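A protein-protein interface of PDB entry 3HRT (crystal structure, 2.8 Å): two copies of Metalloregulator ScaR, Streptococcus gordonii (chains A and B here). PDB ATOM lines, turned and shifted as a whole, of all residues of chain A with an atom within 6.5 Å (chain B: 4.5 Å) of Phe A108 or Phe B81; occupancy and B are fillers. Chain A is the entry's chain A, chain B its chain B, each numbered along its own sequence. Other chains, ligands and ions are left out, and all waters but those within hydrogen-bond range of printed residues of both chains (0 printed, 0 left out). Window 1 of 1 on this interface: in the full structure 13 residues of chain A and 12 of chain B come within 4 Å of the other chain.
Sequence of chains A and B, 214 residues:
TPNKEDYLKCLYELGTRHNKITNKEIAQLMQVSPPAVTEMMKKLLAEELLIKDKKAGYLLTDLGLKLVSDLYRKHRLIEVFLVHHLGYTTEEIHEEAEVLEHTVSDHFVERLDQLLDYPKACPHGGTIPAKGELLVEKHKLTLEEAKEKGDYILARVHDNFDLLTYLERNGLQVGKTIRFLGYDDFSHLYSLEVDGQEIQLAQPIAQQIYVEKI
NE of Arg A111 is in hydrogen-bond range of O of Leu B86, at 3.1 Å. The side-chain carboxylate (OE2) of Glu B96 is in hydrogen-bond range of a ring nitrogen (ND1) of His A107 (3.4 Å). OE1 of Glu B96 sits at hydrogen-bond distance from OG of Ser A105.
The side-chain hydroxyl (OG) of Ser A105 is in hydrogen-bond range of the backbone NH (N) of Phe A108. O of Phe B81 sits at hydrogen-bond distance from N of Leu B86, at 3.3 Å. The backbone carbonyl oxygen (O) of Leu B82 is in hydrogen-bond range of the backbone NH (N) of Tyr B88, at 3.0 Å. OG of Ser A105 is in hydrogen-bond range of N of His A107, 3.2 Å away. The side-chain carboxylate (OE1) of Glu B96 sits at hydrogen-bond distance from the side-chain hydroxyl (OH) of Tyr B88.
Among the printed residues, merely in contact across the chains: Phe A81 with Phe B81, His A107 with Tyr B88, Phe A108 with Phe B81, Phe A108 with Leu B82, Phe A108 with Leu B86, Phe A108 with Tyr B88, Phe A108 with Glu B96, Leu A115 with Phe B81 and Leu A115 with Leu B86.
Printed residues of chain B within 4 Å of Ser A105: Glu B96. Phe A108 touches five residues of chain B. Printed residues of chain B within 4 Å of Leu A115: Phe B81 and Leu B86. Phe B81 touches just these residues of chain A: Phe A81 (3.8 Å), Phe A108 (3.97 Å) and Leu A115 (3.8 Å). Of the printed residues of chain A, Leu B86 touches Phe A108, Arg A111 and Leu A115. The nearest residue of chain A that does not touch Phe B81 is Leu A112 (4.7 Å).
Hydrophobic or aromatic side chains of chain B within 4 Å of the printed part of chain A: Phe B81, Leu B82, Leu B86 and Tyr B88. Hydrophobic or aromatic side chains of chain A that line the printed part of chain B: Phe A81, His A107, Phe A108 and Leu A115. Among the printed residues, 12 pairs touch across the chains.
Phe A81 touches its own counterpart, Phe B81. Positions printed for both chains: 78, 81, 85 and 112.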
ATOM      1  N   ILE A  78     -11.606   2.777  24.483  1.00  0.00           N
ATOM      2  CA  ILE A  78     -12.578   3.751  24.018  1.00  0.00           C
ATOM      3  C   ILE A  78     -12.192   5.167  24.453  1.00  0.00           C
ATOM      4  O   ILE A  78     -12.216   6.114  23.653  1.00  0.00           O
ATOM      5  CB  ILE A  78     -14.007   3.451  24.506  1.00  0.00           C
ATOM      6  CG1 ILE A  78     -14.535   2.156  23.879  1.00  0.00           C
ATOM      7  CG2 ILE A  78     -14.936   4.610  24.185  1.00  0.00           C
ATOM      8  CD1 ILE A  78     -14.338   2.067  22.387  1.00  0.00           C
ATOM      9  N   PHE A  81      -9.183   6.588  22.458  1.00  0.00           N
ATOM     10  CA  PHE A  81      -9.608   6.983  21.123  1.00  0.00           C
ATOM     11  C   PHE A  81     -10.397   8.305  21.133  1.00  0.00           C
ATOM     12  O   PHE A  81     -10.030   9.236  20.426  1.00  0.00           O
ATOM     13  CB  PHE A  81     -10.382   5.831  20.433  1.00  0.00           C
ATOM     14  CG  PHE A  81     -11.118   6.251  19.184  1.00  0.00           C
ATOM     15  CD1 PHE A  81     -10.425   6.570  18.025  1.00  0.00           C
ATOM     16  CD2 PHE A  81     -12.495   6.341  19.175  1.00  0.00           C
ATOM     17  CE1 PHE A  81     -11.086   6.960  16.891  1.00  0.00           C
ATOM     18  CE2 PHE A  81     -13.163   6.739  18.041  1.00  0.00           C
ATOM     19  CZ  PHE A  81     -12.457   7.053  16.900  1.00  0.00           C
ATOM     20  N   HIS A  85      -7.899  10.864  19.637  1.00  0.00           N
ATOM     21  CA  HIS A  85      -8.275  10.904  18.223  1.00  0.00           C
ATOM     22  C   HIS A  85      -9.355  11.954  17.944  1.00  0.00           C
ATOM     23  O   HIS A  85      -9.226  12.713  17.001  1.00  0.00           O
ATOM     24  CB  HIS A  85      -8.638   9.503  17.690  1.00  0.00           C
ATOM     25  CG  HIS A  85      -7.441   8.653  17.384  1.00  0.00           C
ATOM     26  ND1 HIS A  85      -7.414   7.728  16.360  1.00  0.00           N
ATOM     27  CD2 HIS A  85      -6.215   8.605  17.961  1.00  0.00           C
ATOM     28  CE1 HIS A  85      -6.225   7.147  16.324  1.00  0.00           C
ATOM     29  NE2 HIS A  85      -5.482   7.653  17.293  1.00  0.00           N
ATOM     30  N   LEU A 100     -21.279   3.778  23.938  1.00  0.00           N
ATOM     31  CA  LEU A 100     -20.406   3.166  22.951  1.00  0.00           C
ATOM     32  C   LEU A 100     -19.774   1.898  23.490  1.00  0.00           C
ATOM     33  O   LEU A 100     -19.455   0.999  22.724  1.00  0.00           O
ATOM     34  CB  LEU A 100     -19.313   4.135  22.517  1.00  0.00           C
ATOM     35  CG  LEU A 100     -19.641   5.106  21.391  1.00  0.00           C
ATOM     36  CD1 LEU A 100     -20.544   6.251  21.885  1.00  0.00           C
ATOM     37  CD2 LEU A 100     -18.343   5.640  20.799  1.00  0.00           C
ATOM     38  N   VAL A 104     -20.164  -1.722  21.038  1.00  0.00           N
ATOM     39  CA  VAL A 104     -19.135  -2.234  20.126  1.00  0.00           C
ATOM     40  C   VAL A 104     -18.753  -3.696  20.355  1.00  0.00           C
ATOM     41  O   VAL A 104     -18.591  -4.171  21.496  1.00  0.00           O
ATOM     42  CB  VAL A 104     -17.835  -1.404  20.176  1.00  0.00           C
ATOM     43  CG1 VAL A 104     -18.136   0.055  19.974  1.00  0.00           C
ATOM     44  CG2 VAL A 104     -17.085  -1.651  21.508  1.00  0.00           C
ATOM     45  N   SER A 105     -18.598  -4.398  19.235  1.00  0.00           N
ATOM     46  CA  SER A 105     -18.119  -5.772  19.242  1.00  0.00           C
ATOM     47  C   SER A 105     -16.709  -5.833  19.820  1.00  0.00           C
ATOM     48  O   SER A 105     -16.084  -4.804  20.037  1.00  0.00           O
ATOM     49  CB  SER A 105     -18.092  -6.317  17.821  1.00  0.00           C
ATOM     50  OG  SER A 105     -16.971  -5.821  17.116  1.00  0.00           O
ATOM     51  N   ASP A 106     -16.207  -7.036  20.047  1.00  0.00           N
ATOM     52  CA  ASP A 106     -14.849  -7.206  20.509  1.00  0.00           C
ATOM     53  C   ASP A 106     -13.837  -7.116  19.360  1.00  0.00           C
ATOM     54  O   ASP A 106     -12.669  -6.825  19.588  1.00  0.00           O
ATOM     55  CB  ASP A 106     -14.731  -8.509  21.297  1.00  0.00           C
ATOM     56  CG  ASP A 106     -15.632  -8.521  22.544  1.00  0.00           C
ATOM     57  OD1 ASP A 106     -15.992  -7.412  23.034  1.00  0.00           O
ATOM     58  OD2 ASP A 106     -15.982  -9.634  23.023  1.00  0.00           O
ATOM     59  N   HIS A 107     -14.293  -7.327  18.128  1.00  0.00           N
ATOM     60  CA  HIS A 107     -13.458  -7.140  16.939  1.00  0.00           C
ATOM     61  C   HIS A 107     -13.194  -5.637  16.757  1.00  0.00           C
ATOM     62  O   HIS A 107     -12.139  -5.216  16.281  1.00  0.00           O
ATOM     63  CB  HIS A 107     -14.168  -7.735  15.722  1.00  0.00           C
ATOM     64  CG  HIS A 107     -13.396  -7.640  14.437  1.00  0.00           C
ATOM     65  ND1 HIS A 107     -13.752  -6.788  13.408  1.00  0.00           N
ATOM     66  CD2 HIS A 107     -12.308  -8.324  13.996  1.00  0.00           C
ATOM     67  CE1 HIS A 107     -12.909  -6.931  12.401  1.00  0.00           C
ATOM     68  NE2 HIS A 107     -12.027  -7.861  12.726  1.00  0.00           N
ATOM     69  N   PHE A 108     -14.162  -4.820  17.141  1.00  0.00           N
ATOM     70  CA  PHE A 108     -14.002  -3.397  16.995  1.00  0.00           C
ATOM     71  C   PHE A 108     -12.853  -3.041  17.899  1.00  0.00           C
ATOM     72  O   PHE A 108     -11.940  -2.303  17.529  1.00  0.00           O
ATOM     73  CB  PHE A 108     -15.253  -2.678  17.469  1.00  0.00           C
ATOM     74  CG  PHE A 108     -15.135  -1.200  17.422  1.00  0.00           C
ATOM     75  CD1 PHE A 108     -15.212  -0.523  16.220  1.00  0.00           C
ATOM     76  CD2 PHE A 108     -14.921  -0.482  18.566  1.00  0.00           C
ATOM     77  CE1 PHE A 108     -15.079   0.876  16.170  1.00  0.00           C
ATOM     78  CE2 PHE A 108     -14.795   0.915  18.523  1.00  0.00           C
ATOM     79  CZ  PHE A 108     -14.873   1.593  17.323  1.00  0.00           C
ATOM     80  N   VAL A 109     -12.896  -3.621  19.090  1.00  0.00           N
ATOM     81  CA  VAL A 109     -11.963  -3.289  20.134  1.00  0.00           C
ATOM     82  C   VAL A 109     -10.573  -3.873  19.864  1.00  0.00           C
ATOM     83  O   VAL A 109      -9.570  -3.196  20.101  1.00  0.00           O
ATOM     84  CB  VAL A 109     -12.506  -3.722  21.501  1.00  0.00           C
ATOM     85  CG1 VAL A 109     -11.471  -3.497  22.589  1.00  0.00           C
ATOM     86  CG2 VAL A 109     -13.797  -2.973  21.799  1.00  0.00           C
ATOM     87  N   GLU A 110     -10.491  -5.102  19.358  1.00  0.00           N
ATOM     88  CA  GLU A 110      -9.172  -5.683  19.075  1.00  0.00           C
ATOM     89  C   GLU A 110      -8.498  -4.939  17.933  1.00  0.00           C
ATOM     90  O   GLU A 110      -7.300  -5.084  17.706  1.00  0.00           O
ATOM     91  CB  GLU A 110      -9.242  -7.190  18.761  1.00  0.00           C
ATOM     92  CG  GLU A 110      -9.590  -8.109  19.978  1.00  0.00           C
ATOM     93  CD  GLU A 110      -8.754  -7.831  21.261  1.00  0.00           C
ATOM     94  OE1 GLU A 110      -9.354  -7.539  22.337  1.00  0.00           O
ATOM     95  OE2 GLU A 110      -7.499  -7.894  21.193  1.00  0.00           O
ATOM     96  N   ARG A 111      -9.280  -4.143  17.212  1.00  0.00           N
ATOM     97  CA  ARG A 111      -8.770  -3.452  16.044  1.00  0.00           C
ATOM     98  C   ARG A 111      -8.526  -2.001  16.411  1.00  0.00           C
ATOM     99  O   ARG A 111      -7.590  -1.368  15.923  1.00  0.00           O
ATOM    100  CB  ARG A 111      -9.750  -3.556  14.874  1.00  0.00           C
ATOM    101  CG  ARG A 111      -9.715  -4.874  14.104  1.00  0.00           C
ATOM    102  CD  ARG A 111      -8.428  -5.045  13.300  1.00  0.00           C
ATOM    103  NE  ARG A 111      -8.659  -5.785  12.062  1.00  0.00           N
ATOM    104  CZ  ARG A 111      -7.728  -6.454  11.377  1.00  0.00           C
ATOM    105  NH1 ARG A 111      -6.473  -6.493  11.814  1.00  0.00           N
ATOM    106  NH2 ARG A 111      -8.061  -7.097  10.250  1.00  0.00           N
ATOM    107  N   LEU A 112      -9.377  -1.477  17.285  1.00  0.00           N
ATOM    108  CA  LEU A 112      -9.164  -0.166  17.874  1.00  0.00           C
ATOM    109  C   LEU A 112      -7.809  -0.126  18.527  1.00  0.00           C
ATOM    110  O   LEU A 112      -7.136   0.896  18.503  1.00  0.00           O
ATOM    111  CB  LEU A 112     -10.181   0.066  18.956  1.00  0.00           C
ATOM    112  CG  LEU A 112     -10.839   1.424  18.924  1.00  0.00           C
ATOM    113  CD1 LEU A 112     -11.106   1.864  20.361  1.00  0.00           C
ATOM    114  CD2 LEU A 112      -9.993   2.427  18.148  1.00  0.00           C
ATOM    115  N   ASP A 113      -7.425  -1.248  19.122  1.00  0.00           N
ATOM    116  CA  ASP A 113      -6.161  -1.369  19.824  1.00  0.00           C
ATOM    117  C   ASP A 113      -5.022  -1.227  18.849  1.00  0.00           C
ATOM    118  O   ASP A 113      -4.184  -0.361  19.015  1.00  0.00           O
ATOM    119  CB  ASP A 113      -6.067  -2.725  20.527  1.00  0.00           C
ATOM    120  CG  ASP A 113      -4.929  -2.790  21.539  1.00  0.00           C
ATOM    121  OD1 ASP A 113      -4.655  -1.768  22.204  1.00  0.00           O
ATOM    122  OD2 ASP A 113      -4.327  -3.871  21.686  1.00  0.00           O
ATOM    123  N   LEU A 115      -4.999   0.086  16.080  1.00  0.00           N
ATOM    124  CA  LEU A 115      -5.008   1.444  15.545  1.00  0.00           C
ATOM    125  C   LEU A 115      -4.302   2.418  16.519  1.00  0.00           C
ATOM    126  O   LEU A 115      -3.478   3.248  16.087  1.00  0.00           O
ATOM    127  CB  LEU A 115      -6.436   1.886  15.152  1.00  0.00           C
ATOM    128  CG  LEU A 115      -6.640   3.382  14.887  1.00  0.00           C
ATOM    129  CD1 LEU A 115      -5.781   3.857  13.752  1.00  0.00           C
ATOM    130  CD2 LEU A 115      -8.103   3.773  14.669  1.00  0.00           C
ATOM    131  N   LEU B  77     -19.148   7.920   6.341  1.00  0.00           N
ATOM    132  CA  LEU B  77     -18.006   8.145   7.245  1.00  0.00           C
ATOM    133  C   LEU B  77     -17.707   6.918   8.136  1.00  0.00           C
ATOM    134  O   LEU B  77     -16.559   6.492   8.246  1.00  0.00           O
ATOM    135  CB  LEU B  77     -18.244   9.377   8.118  1.00  0.00           C
ATOM    136  CG  LEU B  77     -18.344  10.738   7.424  1.00  0.00           C
ATOM    137  CD1 LEU B  77     -19.017  11.761   8.321  1.00  0.00           C
ATOM    138  CD2 LEU B  77     -16.991  11.249   6.959  1.00  0.00           C
ATOM    139  N   ILE B  78     -18.734   6.353   8.769  1.00  0.00           N
ATOM    140  CA  ILE B  78     -18.557   5.161   9.590  1.00  0.00           C
ATOM    141  C   ILE B  78     -17.913   4.037   8.797  1.00  0.00           C
ATOM    142  O   ILE B  78     -17.102   3.281   9.322  1.00  0.00           O
ATOM    143  CB  ILE B  78     -19.892   4.641  10.112  1.00  0.00           C
ATOM    144  CG1 ILE B  78     -20.472   5.599  11.148  1.00  0.00           C
ATOM    145  CG2 ILE B  78     -19.726   3.255  10.694  1.00  0.00           C
ATOM    146  CD1 ILE B  78     -20.016   5.345  12.534  1.00  0.00           C
ATOM    147  N   GLU B  79     -18.295   3.916   7.536  1.00  0.00           N
ATOM    148  CA  GLU B  79     -17.709   2.908   6.673  1.00  0.00           C
ATOM    149  C   GLU B  79     -16.242   3.221   6.378  1.00  0.00           C
ATOM    150  O   GLU B  79     -15.396   2.324   6.386  1.00  0.00           O
ATOM    151  CB  GLU B  79     -18.500   2.793   5.366  1.00  0.00           C
ATOM    152  CG  GLU B  79     -19.565   1.714   5.382  1.00  0.00           C
ATOM    153  CD  GLU B  79     -20.093   1.401   3.985  1.00  0.00           C
ATOM    154  OE1 GLU B  79     -20.099   2.324   3.148  1.00  0.00           O
ATOM    155  OE2 GLU B  79     -20.507   0.247   3.716  1.00  0.00           O
ATOM    156  N   VAL B  80     -15.948   4.494   6.117  1.00  0.00           N
ATOM    157  CA  VAL B  80     -14.597   4.916   5.777  1.00  0.00           C
ATOM    158  C   VAL B  80     -13.638   4.592   6.934  1.00  0.00           C
ATOM    159  O   VAL B  80     -12.561   4.026   6.727  1.00  0.00           O
ATOM    160  CB  VAL B  80     -14.555   6.414   5.518  1.00  0.00           C
ATOM    161  CG1 VAL B  80     -13.182   6.841   5.022  1.00  0.00           C
ATOM    162  CG2 VAL B  80     -15.637   6.804   4.544  1.00  0.00           C
ATOM    163  N   PHE B  81     -14.045   4.949   8.152  1.00  0.00           N
ATOM    164  CA  PHE B  81     -13.273   4.680   9.351  1.00  0.00           C
ATOM    165  C   PHE B  81     -13.053   3.191   9.501  1.00  0.00           C
ATOM    166  O   PHE B  81     -11.918   2.732   9.529  1.00  0.00           O
ATOM    167  CB  PHE B  81     -14.003   5.231  10.588  1.00  0.00           C
ATOM    168  CG  PHE B  81     -13.328   4.900  11.899  1.00  0.00           C
ATOM    169  CD1 PHE B  81     -12.113   5.483  12.242  1.00  0.00           C
ATOM    170  CD2 PHE B  81     -13.911   4.011  12.795  1.00  0.00           C
ATOM    171  CE1 PHE B  81     -11.477   5.165  13.453  1.00  0.00           C
ATOM    172  CE2 PHE B  81     -13.279   3.688  14.025  1.00  0.00           C
ATOM    173  CZ  PHE B  81     -12.065   4.268  14.347  1.00  0.00           C
ATOM    174  N   LEU B  82     -14.149   2.446   9.587  1.00  0.00           N
ATOM    175  CA  LEU B  82     -14.107   1.005   9.775  1.00  0.00           C
ATOM    176  C   LEU B  82     -13.338   0.282   8.672  1.00  0.00           C
ATOM    177  O   LEU B  82     -12.676  -0.720   8.934  1.00  0.00           O
ATOM    178  CB  LEU B  82     -15.525   0.444   9.840  1.00  0.00           C
ATOM    179  CG  LEU B  82     -16.376   0.859  11.031  1.00  0.00           C
ATOM    180  CD1 LEU B  82     -17.749   0.243  10.915  1.00  0.00           C
ATOM    181  CD2 LEU B  82     -15.718   0.465  12.362  1.00  0.00           C
ATOM    182  N   VAL B  83     -13.439   0.768   7.437  1.00  0.00           N
ATOM    183  CA  VAL B  83     -12.756   0.098   6.340  1.00  0.00           C
ATOM    184  C   VAL B  83     -11.308   0.536   6.202  1.00  0.00           C
ATOM    185  O   VAL B  83     -10.414  -0.301   6.184  1.00  0.00           O
ATOM    186  CB  VAL B  83     -13.506   0.221   4.984  1.00  0.00           C
ATOM    187  CG1 VAL B  83     -12.579  -0.125   3.831  1.00  0.00           C
ATOM    188  CG2 VAL B  83     -14.734  -0.690   4.976  1.00  0.00           C
ATOM    189  N   HIS B  84     -11.075   1.838   6.102  1.00  0.00           N
ATOM    190  CA  HIS B  84      -9.708   2.352   6.023  1.00  0.00           C
ATOM    191  C   HIS B  84      -8.794   2.095   7.244  1.00  0.00           C
ATOM    192  O   HIS B  84      -7.609   1.775   7.079  1.00  0.00           O
ATOM    193  CB  HIS B  84      -9.722   3.844   5.725  1.00  0.00           C
ATOM    194  CG  HIS B  84      -9.808   4.156   4.270  1.00  0.00           C
ATOM    195  ND1 HIS B  84     -10.466   5.264   3.785  1.00  0.00           N
ATOM    196  CD2 HIS B  84      -9.325   3.497   3.194  1.00  0.00           C
ATOM    197  CE1 HIS B  84     -10.374   5.280   2.469  1.00  0.00           C
ATOM    198  NE2 HIS B  84      -9.692   4.216   2.086  1.00  0.00           N
ATOM    199  N   HIS B  85      -9.325   2.243   8.457  1.00  0.00           N
ATOM    200  CA  HIS B  85      -8.461   2.231   9.630  1.00  0.00           C
ATOM    201  C   HIS B  85      -8.588   1.042  10.571  1.00  0.00           C
ATOM    202  O   HIS B  85      -7.597   0.621  11.148  1.00  0.00           O
ATOM    203  CB  HIS B  85      -8.534   3.564  10.375  1.00  0.00           C
ATOM    204  CG  HIS B  85      -7.984   4.705   9.583  1.00  0.00           C
ATOM    205  ND1 HIS B  85      -8.788   5.587   8.896  1.00  0.00           N
ATOM    206  CD2 HIS B  85      -6.709   5.076   9.326  1.00  0.00           C
ATOM    207  CE1 HIS B  85      -8.032   6.466   8.260  1.00  0.00           C
ATOM    208  NE2 HIS B  85      -6.767   6.173   8.501  1.00  0.00           N
ATOM    209  N   LEU B  86      -9.782   0.492  10.738  1.00  0.00           N
ATOM    210  CA  LEU B  86      -9.874  -0.763  11.482  1.00  0.00           C
ATOM    211  C   LEU B  86      -9.715  -1.965  10.540  1.00  0.00           C
ATOM    212  O   LEU B  86      -9.760  -3.116  10.972  1.00  0.00           O
ATOM    213  CB  LEU B  86     -11.158  -0.875  12.313  1.00  0.00           C
ATOM    214  CG  LEU B  86     -11.705   0.337  13.069  1.00  0.00           C
ATOM    215  CD1 LEU B  86     -12.495  -0.087  14.245  1.00  0.00           C
ATOM    216  CD2 LEU B  86     -10.639   1.277  13.507  1.00  0.00           C
ATOM    217  N   TYR B  88     -11.583  -3.430   8.082  1.00  0.00           N
ATOM    218  CA  TYR B  88     -12.681  -4.375   8.002  1.00  0.00           C
ATOM    219  C   TYR B  88     -12.759  -4.951   6.618  1.00  0.00           C
ATOM    220  O   TYR B  88     -12.069  -4.502   5.704  1.00  0.00           O
ATOM    221  CB  TYR B  88     -13.996  -3.684   8.310  1.00  0.00           C
ATOM    222  CG  TYR B  88     -14.295  -3.621   9.767  1.00  0.00           C
ATOM    223  CD1 TYR B  88     -13.277  -3.540  10.692  1.00  0.00           C
ATOM    224  CD2 TYR B  88     -15.600  -3.646  10.221  1.00  0.00           C
ATOM    225  CE1 TYR B  88     -13.545  -3.487  12.029  1.00  0.00           C
ATOM    226  CE2 TYR B  88     -15.885  -3.594  11.561  1.00  0.00           C
ATOM    227  CZ  TYR B  88     -14.852  -3.514  12.465  1.00  0.00           C
ATOM    228  OH  TYR B  88     -15.134  -3.453  13.810  1.00  0.00           O
ATOM    229  N   GLU B  96     -21.447  -5.251  12.020  1.00  0.00           N
ATOM    230  CA  GLU B  96     -21.317  -4.167  12.992  1.00  0.00           C
ATOM    231  C   GLU B  96     -21.790  -2.792  12.532  1.00  0.00           C
ATOM    232  O   GLU B  96     -22.365  -2.031  13.316  1.00  0.00           O
ATOM    233  CB  GLU B  96     -19.860  -4.048  13.437  1.00  0.00           C
ATOM    234  CG  GLU B  96     -19.209  -5.365  13.813  1.00  0.00           C
ATOM    235  CD  GLU B  96     -17.803  -5.164  14.329  1.00  0.00           C
ATOM    236  OE1 GLU B  96     -17.526  -4.063  14.878  1.00  0.00           O
ATOM    237  OE2 GLU B  96     -16.985  -6.104  14.189  1.00  0.00           O
ATOM    238  N   LEU B 112     -15.163  12.638  13.775  1.00  0.00           N
ATOM    239  CA  LEU B 112     -14.760  11.519  12.927  1.00  0.00           C
ATOM    240  C   LEU B 112     -14.446  12.042  11.546  1.00  0.00           C
ATOM    241  O   LEU B 112     -13.500  11.601  10.900  1.00  0.00           O
ATOM    242  CB  LEU B 112     -15.898  10.523  12.793  1.00  0.00           C
ATOM    243  CG  LEU B 112     -15.497   9.054  12.749  1.00  0.00           C
ATOM    244  CD1 LEU B 112     -16.297   8.363  11.658  1.00  0.00           C
ATOM    245  CD2 LEU B 112     -13.999   8.888  12.504  1.00  0.00           C
ATOM    246  N   LEU B 116     -10.694  12.001   9.818  1.00  0.00           N
ATOM    247  CA  LEU B 116     -10.452  11.426   8.497  1.00  0.00           C
ATOM    248  C   LEU B 116     -10.158  12.461   7.409  1.00  0.00           C
ATOM    249  O   LEU B 116     -10.159  12.148   6.210  1.00  0.00           O
ATOM    250  CB  LEU B 116     -11.669  10.628   8.077  1.00  0.00           C
ATOM    251  CG  LEU B 116     -12.027   9.543   9.064  1.00  0.00           C
ATOM    252  CD1 LEU B 116     -13.407   9.040   8.717  1.00  0.00           C
ATOM    253  CD2 LEU B 116     -10.987   8.444   8.974  1.00  0.00           C
